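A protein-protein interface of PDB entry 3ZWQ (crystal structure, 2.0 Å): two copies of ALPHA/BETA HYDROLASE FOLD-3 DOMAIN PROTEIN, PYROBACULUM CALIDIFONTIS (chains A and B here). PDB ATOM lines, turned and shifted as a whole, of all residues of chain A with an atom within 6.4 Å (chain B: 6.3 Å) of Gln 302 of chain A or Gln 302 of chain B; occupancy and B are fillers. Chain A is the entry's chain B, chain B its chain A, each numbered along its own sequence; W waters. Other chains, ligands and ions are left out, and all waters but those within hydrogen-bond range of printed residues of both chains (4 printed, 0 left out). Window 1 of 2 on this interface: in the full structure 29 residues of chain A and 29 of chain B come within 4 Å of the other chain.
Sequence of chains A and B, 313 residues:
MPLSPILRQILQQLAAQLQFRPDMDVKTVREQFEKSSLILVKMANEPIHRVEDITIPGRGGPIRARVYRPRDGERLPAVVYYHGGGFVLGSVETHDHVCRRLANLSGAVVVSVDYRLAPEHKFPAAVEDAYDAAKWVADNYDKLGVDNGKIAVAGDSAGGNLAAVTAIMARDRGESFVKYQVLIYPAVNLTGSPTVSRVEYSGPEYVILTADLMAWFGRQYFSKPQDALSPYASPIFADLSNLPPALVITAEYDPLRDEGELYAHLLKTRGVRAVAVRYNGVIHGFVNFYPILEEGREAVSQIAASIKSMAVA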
ATOM      1  N   LEU A 247     -14.320 -11.386   9.054  1.00  0.00           N
ATOM      2  CA  LEU A 247     -13.052 -11.210   9.780  1.00  0.00           C
ATOM      3  C   LEU A 247     -13.009  -9.741  10.196  1.00  0.00           C
ATOM      4  O   LEU A 247     -13.143  -8.858   9.355  1.00  0.00           O
ATOM      5  CB  LEU A 247     -11.850 -11.550   8.900  1.00  0.00           C
ATOM      6  CG  LEU A 247     -10.441 -11.286   9.466  1.00  0.00           C
ATOM      7  CD1 LEU A 247     -10.202 -12.130  10.706  1.00  0.00           C
ATOM      8  CD2 LEU A 247      -9.390 -11.551   8.402  1.00  0.00           C
ATOM      9  N   ILE A 249     -10.648  -6.970  11.994  1.00  0.00           N
ATOM     10  CA  ILE A 249      -9.311  -6.611  12.461  1.00  0.00           C
ATOM     11  C   ILE A 249      -9.480  -5.372  13.336  1.00  0.00           C
ATOM     12  O   ILE A 249     -10.147  -4.423  12.929  1.00  0.00           O
ATOM     13  CB  ILE A 249      -8.364  -6.224  11.292  1.00  0.00           C
ATOM     14  CG1 ILE A 249      -8.175  -7.391  10.294  1.00  0.00           C
ATOM     15  CG2 ILE A 249      -7.028  -5.748  11.827  1.00  0.00           C
ATOM     16  CD1 ILE A 249      -7.823  -8.694  10.944  1.00  0.00           C
ATOM     17  N   VAL A 275     -14.657 -13.791  13.396  1.00  0.00           N
ATOM     18  CA  VAL A 275     -13.437 -13.772  14.187  1.00  0.00           C
ATOM     19  C   VAL A 275     -12.995 -12.330  14.384  1.00  0.00           C
ATOM     20  O   VAL A 275     -13.003 -11.547  13.440  1.00  0.00           O
ATOM     21  CB  VAL A 275     -12.311 -14.539  13.479  1.00  0.00           C
ATOM     22  CG1 VAL A 275     -11.000 -14.437  14.266  1.00  0.00           C
ATOM     23  CG2 VAL A 275     -12.710 -15.987  13.289  1.00  0.00           C
ATOM     24  N   VAL A 277      -9.677 -10.231  15.642  1.00  0.00           N
ATOM     25  CA  VAL A 277      -8.288 -10.297  16.066  1.00  0.00           C
ATOM     26  C   VAL A 277      -7.820  -8.878  16.359  1.00  0.00           C
ATOM     27  O   VAL A 277      -8.169  -7.928  15.643  1.00  0.00           O
ATOM     28  CB  VAL A 277      -7.379 -10.969  15.016  1.00  0.00           C
ATOM     29  CG1 VAL A 277      -8.040 -12.244  14.467  1.00  0.00           C
ATOM     30  CG2 VAL A 277      -7.059 -10.014  13.893  1.00  0.00           C
ATOM     31  N   TYR A 279      -4.606  -6.405  16.714  1.00  0.00           N
ATOM     32  CA  TYR A 279      -3.179  -6.111  16.520  1.00  0.00           C
ATOM     33  C   TYR A 279      -2.704  -5.219  17.663  1.00  0.00           C
ATOM     34  O   TYR A 279      -3.213  -4.119  17.862  1.00  0.00           O
ATOM     35  CB  TYR A 279      -2.921  -5.453  15.144  1.00  0.00           C
ATOM     36  CG  TYR A 279      -2.886  -6.487  14.008  1.00  0.00           C
ATOM     37  CD1 TYR A 279      -4.026  -7.224  13.671  1.00  0.00           C
ATOM     38  CD2 TYR A 279      -1.697  -6.769  13.329  1.00  0.00           C
ATOM     39  CE1 TYR A 279      -3.996  -8.190  12.656  1.00  0.00           C
ATOM     40  CE2 TYR A 279      -1.651  -7.736  12.301  1.00  0.00           C
ATOM     41  CZ  TYR A 279      -2.802  -8.444  11.977  1.00  0.00           C
ATOM     42  OH  TYR A 279      -2.749  -9.404  10.983  1.00  0.00           O
ATOM     43  N   ARG A 297       2.138  -4.903   7.462  1.00  0.00           N
ATOM     44  CA  ARG A 297       2.474  -5.966   6.511  1.00  0.00           C
ATOM     45  C   ARG A 297       1.820  -7.295   6.849  1.00  0.00           C
ATOM     46  O   ARG A 297       1.300  -7.959   5.967  1.00  0.00           O
ATOM     47  CB  ARG A 297       3.995  -6.134   6.387  1.00  0.00           C
ATOM     48  CG  ARG A 297       4.645  -4.994   5.655  1.00  0.00           C
ATOM     49  CD  ARG A 297       6.065  -5.272   5.278  1.00  0.00           C
ATOM     50  NE  ARG A 297       6.959  -5.544   6.407  1.00  0.00           N
ATOM     51  CZ  ARG A 297       7.482  -4.622   7.215  1.00  0.00           C
ATOM     52  NH1 ARG A 297       7.158  -3.337   7.096  1.00  0.00           N
ATOM     53  NH2 ARG A 297       8.317  -4.993   8.171  1.00  0.00           N
ATOM     54  N   GLU A 298       1.871  -7.683   8.124  1.00  0.00           N
ATOM     55  CA  GLU A 298       1.107  -8.812   8.644  1.00  0.00           C
ATOM     56  C   GLU A 298      -0.413  -8.674   8.390  1.00  0.00           C
ATOM     57  O   GLU A 298      -1.048  -9.592   7.856  1.00  0.00           O
ATOM     58  CB  GLU A 298       1.427  -8.993  10.137  1.00  0.00           C
ATOM     59  CG  GLU A 298       0.846 -10.202  10.787  1.00  0.00           C
ATOM     60  CD  GLU A 298       1.181 -11.504  10.051  1.00  0.00           C
ATOM     61  OE1 GLU A 298       2.327 -11.668   9.547  1.00  0.00           O
ATOM     62  OE2 GLU A 298       0.296 -12.368  10.006  1.00  0.00           O
ATOM     63  N   ALA A 299      -1.003  -7.532   8.708  1.00  0.00           N
ATOM     64  CA  ALA A 299      -2.445  -7.351   8.438  1.00  0.00           C
ATOM     65  C   ALA A 299      -2.823  -7.590   6.983  1.00  0.00           C
ATOM     66  O   ALA A 299      -3.799  -8.294   6.716  1.00  0.00           O
ATOM     67  CB  ALA A 299      -2.926  -5.970   8.864  1.00  0.00           C
ATOM     68  N   VAL A 300      -2.104  -6.970   6.039  1.00  0.00           N
ATOM     69  CA  VAL A 300      -2.424  -7.157   4.626  1.00  0.00           C
ATOM     70  C   VAL A 300      -2.282  -8.649   4.292  1.00  0.00           C
ATOM     71  O   VAL A 300      -3.156  -9.217   3.678  1.00  0.00           O
ATOM     72  CB  VAL A 300      -1.552  -6.285   3.669  1.00  0.00           C
ATOM     73  CG1 VAL A 300      -1.936  -6.539   2.217  1.00  0.00           C
ATOM     74  CG2 VAL A 300      -1.706  -4.804   4.013  1.00  0.00           C
ATOM     75  N   SER A 301      -1.205  -9.282   4.740  1.00  0.00           N
ATOM     76  CA  SER A 301      -1.030 -10.730   4.536  1.00  0.00           C
ATOM     77  C   SER A 301      -2.202 -11.564   5.092  1.00  0.00           C
ATOM     78  O   SER A 301      -2.698 -12.467   4.415  1.00  0.00           O
ATOM     79  CB  SER A 301       0.284 -11.205   5.155  1.00  0.00           C
ATOM     80  OG  SER A 301       0.361 -12.610   5.152  1.00  0.00           O
ATOM     81  N   GLN A 302      -2.664 -11.240   6.305  1.00  0.00           N
ATOM     82  CA  GLN A 302      -3.785 -11.969   6.915  1.00  0.00           C
ATOM     83  C   GLN A 302      -5.062 -11.755   6.142  1.00  0.00           C
ATOM     84  O   GLN A 302      -5.770 -12.701   5.845  1.00  0.00           O
ATOM     85  CB  GLN A 302      -4.002 -11.556   8.384  1.00  0.00           C
ATOM     86  CG  GLN A 302      -5.271 -12.144   8.990  1.00  0.00           C
ATOM     87  CD  GLN A 302      -5.470 -11.863  10.492  1.00  0.00           C
ATOM     88  OE1 GLN A 302      -4.949 -10.882  11.070  1.00  0.00           O
ATOM     89  NE2 GLN A 302      -6.255 -12.729  11.122  1.00  0.00           N
ATOM     90  N   ILE A 303      -5.351 -10.504   5.819  1.00  0.00           N
ATOM     91  CA  ILE A 303      -6.560 -10.139   5.078  1.00  0.00           C
ATOM     92  C   ILE A 303      -6.606 -10.800   3.698  1.00  0.00           C
ATOM     93  O   ILE A 303      -7.637 -11.350   3.303  1.00  0.00           O
ATOM     94  CB  ILE A 303      -6.659  -8.609   4.931  1.00  0.00           C
ATOM     95  CG1 ILE A 303      -6.907  -7.979   6.307  1.00  0.00           C
ATOM     96  CG2 ILE A 303      -7.781  -8.196   3.968  1.00  0.00           C
ATOM     97  CD1 ILE A 303      -6.853  -6.460   6.298  1.00  0.00           C
ATOM     98  N   ALA A 304      -5.502 -10.715   2.956  1.00  0.00           N
ATOM     99  CA  ALA A 304      -5.406 -11.369   1.656  1.00  0.00           C
ATOM    100  C   ALA A 304      -5.694 -12.858   1.781  1.00  0.00           C
ATOM    101  O   ALA A 304      -6.508 -13.390   1.033  1.00  0.00           O
ATOM    102  CB  ALA A 304      -4.039 -11.149   1.042  1.00  0.00           C
ATOM    103  N   ALA A 305      -5.039 -13.519   2.731  1.00  0.00           N
ATOM    104  CA  ALA A 305      -5.137 -14.975   2.869  1.00  0.00           C
ATOM    105  C   ALA A 305      -6.517 -15.419   3.339  1.00  0.00           C
ATOM    106  O   ALA A 305      -7.030 -16.433   2.873  1.00  0.00           O
ATOM    107  CB  ALA A 305      -4.069 -15.493   3.804  1.00  0.00           C
ATOM    108  N   SER A 306      -7.116 -14.644   4.239  1.00  0.00           N
ATOM    109  CA  SER A 306      -8.434 -14.964   4.794  1.00  0.00           C
ATOM    110  C   SER A 306      -9.486 -14.894   3.707  1.00  0.00           C
ATOM    111  O   SER A 306     -10.408 -15.702   3.683  1.00  0.00           O
ATOM    112  CB  SER A 306      -8.771 -14.011   5.954  1.00  0.00           C
ATOM    113  OG  SER A 306     -10.057 -14.251   6.501  1.00  0.00           O
ATOM    114  N   ILE A 307      -9.335 -13.926   2.805  1.00  0.00           N
ATOM    115  CA  ILE A 307     -10.209 -13.794   1.652  1.00  0.00           C
ATOM    116  C   ILE A 307      -9.965 -14.950   0.654  1.00  0.00           C
ATOM    117  O   ILE A 307     -10.907 -15.538   0.158  1.00  0.00           O
ATOM    118  CB  ILE A 307     -10.028 -12.408   0.973  1.00  0.00           C
ATOM    119  CG1 ILE A 307     -10.540 -11.293   1.904  1.00  0.00           C
ATOM    120  CG2 ILE A 307     -10.745 -12.357  -0.388  1.00  0.00           C
ATOM    121  CD1 ILE A 307     -10.322  -9.885   1.363  1.00  0.00           C
ATOM    122  N   ALA A 311     -11.354 -18.222   5.078  1.00  0.00           N
ATOM    123  CA  ALA A 311     -10.986 -19.076   6.229  1.00  0.00           C
ATOM    124  C   ALA A 311     -11.996 -19.161   7.374  1.00  0.00           C
ATOM    125  O   ALA A 311     -12.097 -20.200   8.024  1.00  0.00           O
ATOM    126  CB  ALA A 311      -9.623 -18.658   6.799  1.00  0.00           C
ATOM    127  N   LEU B 247       6.179 -13.601  14.315  1.00  0.00           N
ATOM    128  CA  LEU B 247       4.724 -13.479  14.501  1.00  0.00           C
ATOM    129  C   LEU B 247       4.354 -14.232  15.788  1.00  0.00           C
ATOM    130  O   LEU B 247       4.704 -15.404  15.950  1.00  0.00           O
ATOM    131  CB  LEU B 247       3.952 -14.048  13.293  1.00  0.00           C
ATOM    132  CG  LEU B 247       2.419 -14.152  13.437  1.00  0.00           C
ATOM    133  CD1 LEU B 247       1.805 -12.797  13.649  1.00  0.00           C
ATOM    134  CD2 LEU B 247       1.783 -14.842  12.247  1.00  0.00           C
ATOM    135  N   ILE B 249       1.138 -15.270  18.094  1.00  0.00           N
ATOM    136  CA  ILE B 249      -0.310 -15.361  18.153  1.00  0.00           C
ATOM    137  C   ILE B 249      -0.675 -15.573  19.627  1.00  0.00           C
ATOM    138  O   ILE B 249      -0.079 -16.422  20.304  1.00  0.00           O
ATOM    139  CB  ILE B 249      -0.873 -16.553  17.349  1.00  0.00           C
ATOM    140  CG1 ILE B 249      -0.478 -16.493  15.859  1.00  0.00           C
ATOM    141  CG2 ILE B 249      -2.386 -16.629  17.522  1.00  0.00           C
ATOM    142  CD1 ILE B 249      -0.935 -15.278  15.134  1.00  0.00           C
ATOM    143  N   VAL B 275       5.410  -8.928  15.424  1.00  0.00           N
ATOM    144  CA  VAL B 275       3.985  -8.627  15.512  1.00  0.00           C
ATOM    145  C   VAL B 275       3.300  -9.566  16.515  1.00  0.00           C
ATOM    146  O   VAL B 275       3.549 -10.769  16.515  1.00  0.00           O
ATOM    147  CB  VAL B 275       3.319  -8.750  14.145  1.00  0.00           C
ATOM    148  CG1 VAL B 275       1.794  -8.666  14.259  1.00  0.00           C
ATOM    149  CG2 VAL B 275       3.866  -7.673  13.183  1.00  0.00           C
ATOM    150  N   VAL B 277      -0.582 -10.555  17.686  1.00  0.00           N
ATOM    151  CA  VAL B 277      -2.005 -10.478  17.445  1.00  0.00           C
ATOM    152  C   VAL B 277      -2.686 -11.264  18.561  1.00  0.00           C
ATOM    153  O   VAL B 277      -2.120 -12.214  19.089  1.00  0.00           O
ATOM    154  CB  VAL B 277      -2.367 -11.060  16.067  1.00  0.00           C
ATOM    155  CG1 VAL B 277      -3.841 -10.860  15.775  1.00  0.00           C
ATOM    156  CG2 VAL B 277      -1.512 -10.399  14.968  1.00  0.00           C
ATOM    157  N   TYR B 279      -6.205 -13.228  19.370  1.00  0.00           N
ATOM    158  CA  TYR B 279      -7.472 -13.788  18.936  1.00  0.00           C
ATOM    159  C   TYR B 279      -8.449 -13.684  20.088  1.00  0.00           C
ATOM    160  O   TYR B 279      -8.230 -14.248  21.165  1.00  0.00           O
ATOM    161  CB  TYR B 279      -7.292 -15.250  18.471  1.00  0.00           C
ATOM    162  CG  TYR B 279      -6.800 -15.307  17.037  1.00  0.00           C
ATOM    163  CD1 TYR B 279      -5.529 -14.832  16.698  1.00  0.00           C
ATOM    164  CD2 TYR B 279      -7.618 -15.786  16.015  1.00  0.00           C
ATOM    165  CE1 TYR B 279      -5.090 -14.828  15.380  1.00  0.00           C
ATOM    166  CE2 TYR B 279      -7.179 -15.814  14.699  1.00  0.00           C
ATOM    167  CZ  TYR B 279      -5.919 -15.330  14.386  1.00  0.00           C
ATOM    168  OH  TYR B 279      -5.499 -15.338  13.086  1.00  0.00           O
ATOM    169  N   ARG B 297      -9.383 -21.783  12.290  1.00  0.00           N
ATOM    170  CA  ARG B 297      -9.183 -21.729  10.842  1.00  0.00           C
ATOM    171  C   ARG B 297      -8.532 -20.402  10.421  1.00  0.00           C
ATOM    172  O   ARG B 297      -7.582 -20.394   9.641  1.00  0.00           O
ATOM    173  CB  ARG B 297     -10.497 -21.946  10.097  1.00  0.00           C
ATOM    174  CG  ARG B 297     -11.100 -23.342  10.328  1.00  0.00           C
ATOM    175  CD  ARG B 297     -12.224 -23.657   9.374  1.00  0.00           C
ATOM    176  NE  ARG B 297     -13.415 -22.813   9.554  1.00  0.00           N
ATOM    177  CZ  ARG B 297     -14.319 -22.940  10.534  1.00  0.00           C
ATOM    178  NH1 ARG B 297     -14.176 -23.837  11.508  1.00  0.00           N
ATOM    179  NH2 ARG B 297     -15.384 -22.148  10.550  1.00  0.00           N
ATOM    180  N   GLU B 298      -9.026 -19.290  10.956  1.00  0.00           N
ATOM    181  CA  GLU B 298      -8.406 -18.002  10.677  1.00  0.00           C
ATOM    182  C   GLU B 298      -6.937 -18.022  11.076  1.00  0.00           C
ATOM    183  O   GLU B 298      -6.080 -17.643  10.270  1.00  0.00           O
ATOM    184  CB  GLU B 298      -9.155 -16.868  11.354  1.00  0.00           C
ATOM    185  CG  GLU B 298      -8.595 -15.494  11.078  1.00  0.00           C
ATOM    186  CD  GLU B 298      -8.502 -15.152   9.606  1.00  0.00           C
ATOM    187  OE1 GLU B 298      -9.406 -15.533   8.802  1.00  0.00           O
ATOM    188  OE2 GLU B 298      -7.509 -14.487   9.265  1.00  0.00           O
ATOM    189  N   ALA B 299      -6.628 -18.530  12.269  1.00  0.00           N
ATOM    190  CA  ALA B 299      -5.227 -18.625  12.721  1.00  0.00           C
ATOM    191  C   ALA B 299      -4.329 -19.423  11.776  1.00  0.00           C
ATOM    192  O   ALA B 299      -3.219 -18.987  11.476  1.00  0.00           O
ATOM    193  CB  ALA B 299      -5.138 -19.196  14.152  1.00  0.00           C
ATOM    194  N   VAL B 300      -4.760 -20.603  11.328  1.00  0.00           N
ATOM    195  CA  VAL B 300      -3.895 -21.411  10.453  1.00  0.00           C
ATOM    196  C   VAL B 300      -3.672 -20.644   9.137  1.00  0.00           C
ATOM    197  O   VAL B 300      -2.551 -20.577   8.649  1.00  0.00           O
ATOM    198  CB  VAL B 300      -4.442 -22.845  10.214  1.00  0.00           C
ATOM    199  CG1 VAL B 300      -3.532 -23.631   9.256  1.00  0.00           C
ATOM    200  CG2 VAL B 300      -4.585 -23.597  11.552  1.00  0.00           C
ATOM    201  N   SER B 301      -4.732 -20.033   8.605  1.00  0.00           N
ATOM    202  CA  SER B 301      -4.642 -19.182   7.402  1.00  0.00           C
ATOM    203  C   SER B 301      -3.656 -18.025   7.563  1.00  0.00           C
ATOM    204  O   SER B 301      -2.841 -17.763   6.664  1.00  0.00           O
ATOM    205  CB  SER B 301      -6.011 -18.611   7.064  1.00  0.00           C
ATOM    206  OG  SER B 301      -5.944 -17.654   6.031  1.00  0.00           O
ATOM    207  N   GLN B 302      -3.731 -17.333   8.703  1.00  0.00           N
ATOM    208  CA  GLN B 302      -2.803 -16.243   8.976  1.00  0.00           C
ATOM    209  C   GLN B 302      -1.376 -16.740   9.086  1.00  0.00           C
ATOM    210  O   GLN B 302      -0.478 -16.170   8.480  1.00  0.00           O
ATOM    211  CB  GLN B 302      -3.162 -15.507  10.265  1.00  0.00           C
ATOM    212  CG  GLN B 302      -2.053 -14.560  10.698  1.00  0.00           C
ATOM    213  CD  GLN B 302      -2.439 -13.603  11.811  1.00  0.00           C
ATOM    214  OE1 GLN B 302      -3.388 -13.839  12.585  1.00  0.00           O
ATOM    215  NE2 GLN B 302      -1.670 -12.515  11.919  1.00  0.00           N
ATOM    216  N   ILE B 303      -1.168 -17.768   9.898  1.00  0.00           N
ATOM    217  CA  ILE B 303       0.164 -18.303  10.136  1.00  0.00           C
ATOM    218  C   ILE B 303       0.807 -18.775   8.824  1.00  0.00           C
ATOM    219  O   ILE B 303       1.962 -18.451   8.546  1.00  0.00           O
ATOM    220  CB  ILE B 303       0.121 -19.463  11.133  1.00  0.00           C
ATOM    221  CG1 ILE B 303      -0.204 -18.933  12.539  1.00  0.00           C
ATOM    222  CG2 ILE B 303       1.453 -20.247  11.132  1.00  0.00           C
ATOM    223  CD1 ILE B 303      -0.830 -19.972  13.452  1.00  0.00           C
ATOM    224  N   ALA B 304       0.049 -19.563   8.057  1.00  0.00           N
ATOM    225  CA  ALA B 304       0.476 -20.052   6.746  1.00  0.00           C
ATOM    226  C   ALA B 304       0.904 -18.907   5.819  1.00  0.00           C
ATOM    227  O   ALA B 304       1.976 -18.962   5.211  1.00  0.00           O
ATOM    228  CB  ALA B 304      -0.652 -20.860   6.095  1.00  0.00           C
ATOM    229  N   ALA B 305       0.055 -17.884   5.716  1.00  0.00           N
ATOM    230  CA  ALA B 305       0.320 -16.753   4.827  1.00  0.00           C
ATOM    231  C   ALA B 305       1.513 -15.922   5.296  1.00  0.00           C
ATOM    232  O   ALA B 305       2.283 -15.427   4.473  1.00  0.00           O
ATOM    233  CB  ALA B 305      -0.900 -15.879   4.686  1.00  0.00           C
ATOM    234  N   SER B 306       1.665 -15.787   6.617  1.00  0.00           N
ATOM    235  CA  SER B 306       2.744 -14.991   7.181  1.00  0.00           C
ATOM    236  C   SER B 306       4.057 -15.670   6.866  1.00  0.00           C
ATOM    237  O   SER B 306       5.019 -15.010   6.516  1.00  0.00           O
ATOM    238  CB  SER B 306       2.577 -14.789   8.701  1.00  0.00           C
ATOM    239  OG  SER B 306       3.490 -13.821   9.199  1.00  0.00           O
ATOM    240  N   ILE B 307       4.089 -16.993   6.960  1.00  0.00           N
ATOM    241  CA  ILE B 307       5.289 -17.749   6.597  1.00  0.00           C
ATOM    242  C   ILE B 307       5.583 -17.676   5.075  1.00  0.00           C
ATOM    243  O   ILE B 307       6.732 -17.484   4.662  1.00  0.00           O
ATOM    244  CB  ILE B 307       5.170 -19.215   7.058  1.00  0.00           C
ATOM    245  CG1 ILE B 307       5.284 -19.284   8.593  1.00  0.00           C
ATOM    246  CG2 ILE B 307       6.243 -20.101   6.392  1.00  0.00           C
ATOM    247  CD1 ILE B 307       4.840 -20.615   9.181  1.00  0.00           C
HETATM  248  O   HOH W   1      -5.630 -15.248   7.267  1.00  0.00           O
HETATM  249  O   HOH W   2      -0.765 -13.484   7.605  1.00  0.00           O
HETATM  250  O   HOH W   3      -5.762 -19.079   3.441  1.00  0.00           O
HETATM  251  O   HOH W   4       1.209 -13.750   2.389  1.00  0.00           O
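N of Ala 299 of chain B sits close to OH of Tyr 279 of chain B, 3.5 Å away. OH of Tyr 279 of chain B is in hydrogen-bond range of OE1 of Gln 302 of chain B, at 2.6 Å. The side-chain hydroxyl (OH) of Tyr 279 of chain A lies close to the backbone NH (N) of Ala 299 of chain A (3.4 Å). The side-chain hydroxyl of Tyr 279 of chain A lies within hydrogen-bond range of the side-chain amide oxygen of Gln 302 of chain A (2.7 Å). O of Ser 306 of chain A is in hydrogen-bond range of N of Ala 311 of chain A (3.0 Å).
CD2 of Leu 247 of chain A touches OE2 of Glu 298 of chain B, at 3.6 Å. Val 277 of chain A touches Val 277 of chain B. CG1 of Val 277 of chain A touches CE2 of Tyr 279 of chain B (3.7 Å). Glu 298 of chain A touches Leu 247 of chain B (OE2 to CD2, 3.7 Å). CG1 of Val 275 of chain B touches CG of Glu 298 of chain A (3.9 Å). N of Ser 306 of chain B touches OG of Ser 301 of chain A, 3.7 Å away. Ser 301 of chain B touches Ala 305 of chain A. Ala 305 of chain A touches Ala 305 of chain B. Ser 301 of chain B touches Ser 306 of chain A. CB of Ser 301 of chain B touches CB of Ala 311 of chain A, at 3.6 Å.
Of the 17 printed residues of chain A, 9 touch a printed residue of chain B. Printed residues of chain A that touch a printed residue of chain B: Leu 247, Val 277, Tyr 279, Glu 298, Ser 301, Gln 302, Ala 305, Ser 306 and Ala 311. Among the printed residues, no Asp or Glu carboxylate lies within 4 Å of a Lys or Arg side-chain nitrogen of the other chain.
Val 277 of chain A touches its own counterpart, Val 277 of chain B. Ser 301 of chain A touches Ala 305 of chain B, and with the chains exchanged Ala 305 of chain A touches Ser 301 of chain B. Ser 301 of chain A touches Ser 306 of chain B, and with the chains exchanged Ser 306 of chain A touches Ser 301 of chain B. Gln 302 of chain A touches its own counterpart, Gln 302 of chain B. Of the 21 pairs that touch across the chains among the printed residues, 17 have their exchanged pair printed and touching as well.
Water W1 lies within hydrogen-bond range of the side-chain hydroxyl of Ser 301 of chain B (2.7 Å), the side-chain carboxylate of Glu 298 of chain B (2.8 Å), the backbone carbonyl oxygen of Gln 302 of chain A (2.9 Å), the backbone NH of Gln 302 of chain B (3.2 Å) and the backbone NH of Ser 306 of chain A (3.4 Å). Water W2 lies within hydrogen-bond range of OG of Ser 301 of chain A (2.8 Å), O of Gln 302 of chain B (2.8 Å), OE2 of Glu 298 of chain A (2.9 Å), N of Gln 302 of chain A (3.2 Å) and N of Ser 306 of chain B (3.5 Å). Water W4 lies within hydrogen-bond range of O of Ala 305 of chain B and OG of Ser 301 of chain A. Water W3 lies within hydrogen-bond range of OG of Ser 301 of chain B (3.0 Å) and O of Ala 305 of chain A (3.0 Å).
Val 275 of chain A touches none of the printed residues of chain B. Ala 299 of chain A touches none of the printed residues of chain B. Of the printed residues of chain B, Gln 302 of chain A touches Tyr 279, Glu 298 and Gln 302. Of the printed residues of chain A, Leu 247 of chain B touches Glu 298 (3.7 Å). Gln 302 of chain B touches three residues of chain A. Printed residues of chain A within 4 Å of Ala 305 of chain B: Ser 301 and Ala 305.
The side-chain amide nitrogen (NE2) of Gln 302 of chain A lies within hydrogen-bond range of the side-chain hydroxyl (OH) of Tyr 279 of chain B (3.4 Å). The backbone carbonyl oxygen of Ala 311 of chain A lies close to the guanidinium group of Arg 297 of chain B (3.3 Å). NE2 of Gln 302 of chain A sits at hydrogen-bond distance from OE2 of Glu 298 of chain B (2.8 Å). OG of Ser 306 of chain A lies within hydrogen-bond range of OE1 of Glu 298 of chain B (2.7 Å). NE2 of Gln 302 of chain B sits at hydrogen-bond distance from OH of Tyr 279 of chain A (3.4 Å). NE2 of Gln 302 of chain B sits at hydrogen-bond distance from OE2 of Glu 298 of chain A, 2.7 Å away. OE1 of Gln 302 of chain B is in hydrogen-bond range of NE2 of Gln 302 of chain A (3.4 Å). The side-chain hydroxyl of Ser 301 of chain A sits at hydrogen-bond distance from the backbone carbonyl oxygen of Ala 305 of chain B, 3.5 Å away. OG of Ser 306 of chain B is in hydrogen-bond range of OE1 of Glu 298 of chain A.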
